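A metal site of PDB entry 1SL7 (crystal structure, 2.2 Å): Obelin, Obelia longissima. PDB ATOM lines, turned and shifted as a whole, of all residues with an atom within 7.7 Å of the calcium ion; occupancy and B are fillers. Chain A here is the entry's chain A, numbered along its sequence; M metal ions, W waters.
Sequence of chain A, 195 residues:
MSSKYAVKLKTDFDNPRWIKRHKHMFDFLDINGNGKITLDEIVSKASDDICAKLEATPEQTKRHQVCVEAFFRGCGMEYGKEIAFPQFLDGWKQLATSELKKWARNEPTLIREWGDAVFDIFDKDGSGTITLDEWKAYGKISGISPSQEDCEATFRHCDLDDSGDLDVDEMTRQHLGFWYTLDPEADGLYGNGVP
N of Gly 164 lies within hydrogen-bond range of OD2 of Asp 159, at 3.4 Å. The backbone NH (N) of Glu 170 lies within hydrogen-bond range of the side-chain carboxylate (OD1) of Asp 167 (3.1 Å). The side-chain carboxylate of Glu 170 sits close to the backbone NH of Leu 160 (3.4 Å).
Of the 13 residues printed, 5 come within 4 Å of the calcium ion. The nearest printed residue that does not touch the calcium ion is Leu 166 (4.3 Å).
The calcium ion is bound by water W1 (2.3 Å), the side-chain carboxylate (OD1) of Asp 159 (2.4 Å), the backbone carbonyl oxygen (O) of Asp 165 (2.4 Å), the side-chain carboxylate (OE1) of Glu 170 (2.6 Å), the side-chain carboxylate (OD2) of Asp 161 (2.6 Å), the side-chain hydroxyl (OG) of Ser 163 (2.7 Å) and the side-chain carboxylate (OE2) of Glu 170 (2.8 Å).
Water W1 bridges OD2 of Asp 167 (2.9 Å) and OD1 of Asp 161 (3.3 Å).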
ATOM      1  N   ILE A 130      32.199  22.448  14.146  1.00  0.00           N
ATOM      2  CA  ILE A 130      31.251  22.627  15.252  1.00  0.00           C
ATOM      3  C   ILE A 130      29.837  22.872  14.739  1.00  0.00           C
ATOM      4  O   ILE A 130      29.604  23.808  13.956  1.00  0.00           O
ATOM      5  CB  ILE A 130      31.687  23.800  16.197  1.00  0.00           C
ATOM      6  CG1 ILE A 130      33.190  23.731  16.554  1.00  0.00           C
ATOM      7  CG2 ILE A 130      30.796  23.842  17.461  1.00  0.00           C
ATOM      8  CD1 ILE A 130      33.622  22.480  17.267  1.00  0.00           C
ATOM      9  N   PHE A 155      23.956  31.890  16.369  1.00  0.00           N
ATOM     10  CA  PHE A 155      24.735  30.871  15.646  1.00  0.00           C
ATOM     11  C   PHE A 155      24.823  31.159  14.135  1.00  0.00           C
ATOM     12  O   PHE A 155      25.917  31.096  13.547  1.00  0.00           O
ATOM     13  CB  PHE A 155      24.154  29.462  15.877  1.00  0.00           C
ATOM     14  CG  PHE A 155      24.945  28.364  15.198  1.00  0.00           C
ATOM     15  CD1 PHE A 155      26.003  27.742  15.854  1.00  0.00           C
ATOM     16  CD2 PHE A 155      24.640  27.956  13.891  1.00  0.00           C
ATOM     17  CE1 PHE A 155      26.742  26.721  15.236  1.00  0.00           C
ATOM     18  CE2 PHE A 155      25.376  26.954  13.266  1.00  0.00           C
ATOM     19  CZ  PHE A 155      26.424  26.327  13.945  1.00  0.00           C
ATOM     20  N   CYS A 158      27.206  34.018  13.429  1.00  0.00           N
ATOM     21  CA  CYS A 158      28.625  33.612  13.551  1.00  0.00           C
ATOM     22  C   CYS A 158      29.134  32.767  12.369  1.00  0.00           C
ATOM     23  O   CYS A 158      30.312  32.839  11.996  1.00  0.00           O
ATOM     24  CB  CYS A 158      28.861  32.857  14.866  1.00  0.00           C
ATOM     25  SG  CYS A 158      28.560  33.831  16.365  1.00  0.00           S
ATOM     26  N   ASP A 159      28.235  31.965  11.784  1.00  0.00           N
ATOM     27  CA  ASP A 159      28.550  31.154  10.610  1.00  0.00           C
ATOM     28  C   ASP A 159      28.606  32.069   9.388  1.00  0.00           C
ATOM     29  O   ASP A 159      27.592  32.296   8.722  1.00  0.00           O
ATOM     30  CB  ASP A 159      27.496  30.048  10.480  1.00  0.00           C
ATOM     31  CG  ASP A 159      27.579  29.294   9.160  1.00  0.00           C
ATOM     32  OD1 ASP A 159      28.685  28.927   8.710  1.00  0.00           O
ATOM     33  OD2 ASP A 159      26.548  28.997   8.512  1.00  0.00           O
ATOM     34  N   LEU A 160      29.801  32.612   9.114  1.00  0.00           N
ATOM     35  CA  LEU A 160      30.009  33.679   8.119  1.00  0.00           C
ATOM     36  C   LEU A 160      29.566  33.283   6.705  1.00  0.00           C
ATOM     37  O   LEU A 160      28.611  33.872   6.176  1.00  0.00           O
ATOM     38  CB  LEU A 160      31.448  34.219   8.137  1.00  0.00           C
ATOM     39  CG  LEU A 160      31.902  34.999   9.387  1.00  0.00           C
ATOM     40  CD1 LEU A 160      33.417  35.020   9.513  1.00  0.00           C
ATOM     41  CD2 LEU A 160      31.344  36.427   9.433  1.00  0.00           C
ATOM     42  N   ASP A 161      30.255  32.311   6.096  1.00  0.00           N
ATOM     43  CA  ASP A 161      29.718  31.638   4.915  1.00  0.00           C
ATOM     44  C   ASP A 161      28.510  30.844   5.394  1.00  0.00           C
ATOM     45  O   ASP A 161      28.261  30.813   6.592  1.00  0.00           O
ATOM     46  CB  ASP A 161      30.779  30.766   4.193  1.00  0.00           C
ATOM     47  CG  ASP A 161      31.137  29.478   4.960  1.00  0.00           C
ATOM     48  OD1 ASP A 161      32.187  28.871   4.648  1.00  0.00           O
ATOM     49  OD2 ASP A 161      30.436  28.986   5.877  1.00  0.00           O
ATOM     50  N   ASP A 162      27.747  30.211   4.523  1.00  0.00           N
ATOM     51  CA  ASP A 162      26.520  29.563   4.997  1.00  0.00           C
ATOM     52  C   ASP A 162      26.614  28.040   5.031  1.00  0.00           C
ATOM     53  O   ASP A 162      25.628  27.329   4.770  1.00  0.00           O
ATOM     54  CB  ASP A 162      25.305  30.069   4.216  1.00  0.00           C
ATOM     55  CG  ASP A 162      24.999  31.537   4.489  1.00  0.00           C
ATOM     56  OD1 ASP A 162      24.493  31.846   5.590  1.00  0.00           O
ATOM     57  OD2 ASP A 162      25.255  32.435   3.659  1.00  0.00           O
ATOM     58  N   SER A 163      27.800  27.555   5.410  1.00  0.00           N
ATOM     59  CA  SER A 163      28.140  26.133   5.336  1.00  0.00           C
ATOM     60  C   SER A 163      27.346  25.212   6.274  1.00  0.00           C
ATOM     61  O   SER A 163      27.412  23.991   6.144  1.00  0.00           O
ATOM     62  CB  SER A 163      29.642  25.944   5.572  1.00  0.00           C
ATOM     63  OG  SER A 163      29.942  25.940   6.962  1.00  0.00           O
ATOM     64  N   GLY A 164      26.607  25.804   7.227  1.00  0.00           N
ATOM     65  CA  GLY A 164      25.860  25.025   8.208  1.00  0.00           C
ATOM     66  C   GLY A 164      26.603  24.638   9.489  1.00  0.00           C
ATOM     67  O   GLY A 164      26.014  24.030  10.387  1.00  0.00           O
ATOM     68  N   ASP A 165      27.887  25.004   9.576  1.00  0.00           N
ATOM     69  CA  ASP A 165      28.734  24.678  10.734  1.00  0.00           C
ATOM     70  C   ASP A 165      29.904  25.669  10.908  1.00  0.00           C
ATOM     71  O   ASP A 165      30.059  26.584  10.085  1.00  0.00           O
ATOM     72  CB  ASP A 165      29.256  23.224  10.634  1.00  0.00           C
ATOM     73  CG  ASP A 165      29.852  22.897   9.263  1.00  0.00           C
ATOM     74  OD1 ASP A 165      30.166  23.824   8.484  1.00  0.00           O
ATOM     75  OD2 ASP A 165      30.068  21.729   8.879  1.00  0.00           O
ATOM     76  N   LEU A 166      30.698  25.513  11.968  1.00  0.00           N
ATOM     77  CA  LEU A 166      31.831  26.432  12.200  1.00  0.00           C
ATOM     78  C   LEU A 166      33.227  25.817  12.025  1.00  0.00           C
ATOM     79  O   LEU A 166      33.522  24.748  12.561  1.00  0.00           O
ATOM     80  CB  LEU A 166      31.735  27.131  13.580  1.00  0.00           C
ATOM     81  CG  LEU A 166      30.386  27.692  14.060  1.00  0.00           C
ATOM     82  CD1 LEU A 166      30.483  28.124  15.504  1.00  0.00           C
ATOM     83  CD2 LEU A 166      29.866  28.845  13.180  1.00  0.00           C
ATOM     84  N   ASP A 167      34.091  26.495  11.273  1.00  0.00           N
ATOM     85  CA  ASP A 167      35.495  26.115  11.239  1.00  0.00           C
ATOM     86  C   ASP A 167      36.278  26.834  12.339  1.00  0.00           C
ATOM     87  O   ASP A 167      35.681  27.537  13.171  1.00  0.00           O
ATOM     88  CB  ASP A 167      36.121  26.348   9.851  1.00  0.00           C
ATOM     89  CG  ASP A 167      35.894  27.761   9.338  1.00  0.00           C
ATOM     90  OD1 ASP A 167      36.360  28.716   9.992  1.00  0.00           O
ATOM     91  OD2 ASP A 167      35.282  28.023   8.275  1.00  0.00           O
ATOM     92  N   GLU A 170      36.202  30.834  12.257  1.00  0.00           N
ATOM     93  CA  GLU A 170      34.877  31.313  12.708  1.00  0.00           C
ATOM     94  C   GLU A 170      34.655  31.153  14.221  1.00  0.00           C
ATOM     95  O   GLU A 170      34.142  32.073  14.867  1.00  0.00           O
ATOM     96  CB  GLU A 170      33.747  30.630  11.935  1.00  0.00           C
ATOM     97  CG  GLU A 170      33.660  31.007  10.458  1.00  0.00           C
ATOM     98  CD  GLU A 170      32.747  30.092   9.654  1.00  0.00           C
ATOM     99  OE1 GLU A 170      32.385  29.006  10.166  1.00  0.00           O
ATOM    100  OE2 GLU A 170      32.381  30.432   8.507  1.00  0.00           O
HETATM  101 CA    CA M   1      30.847  28.079   8.322  1.00  0.00          CA
HETATM  102  O   HOH W   1      32.684  27.093   7.414  1.00  0.00           O
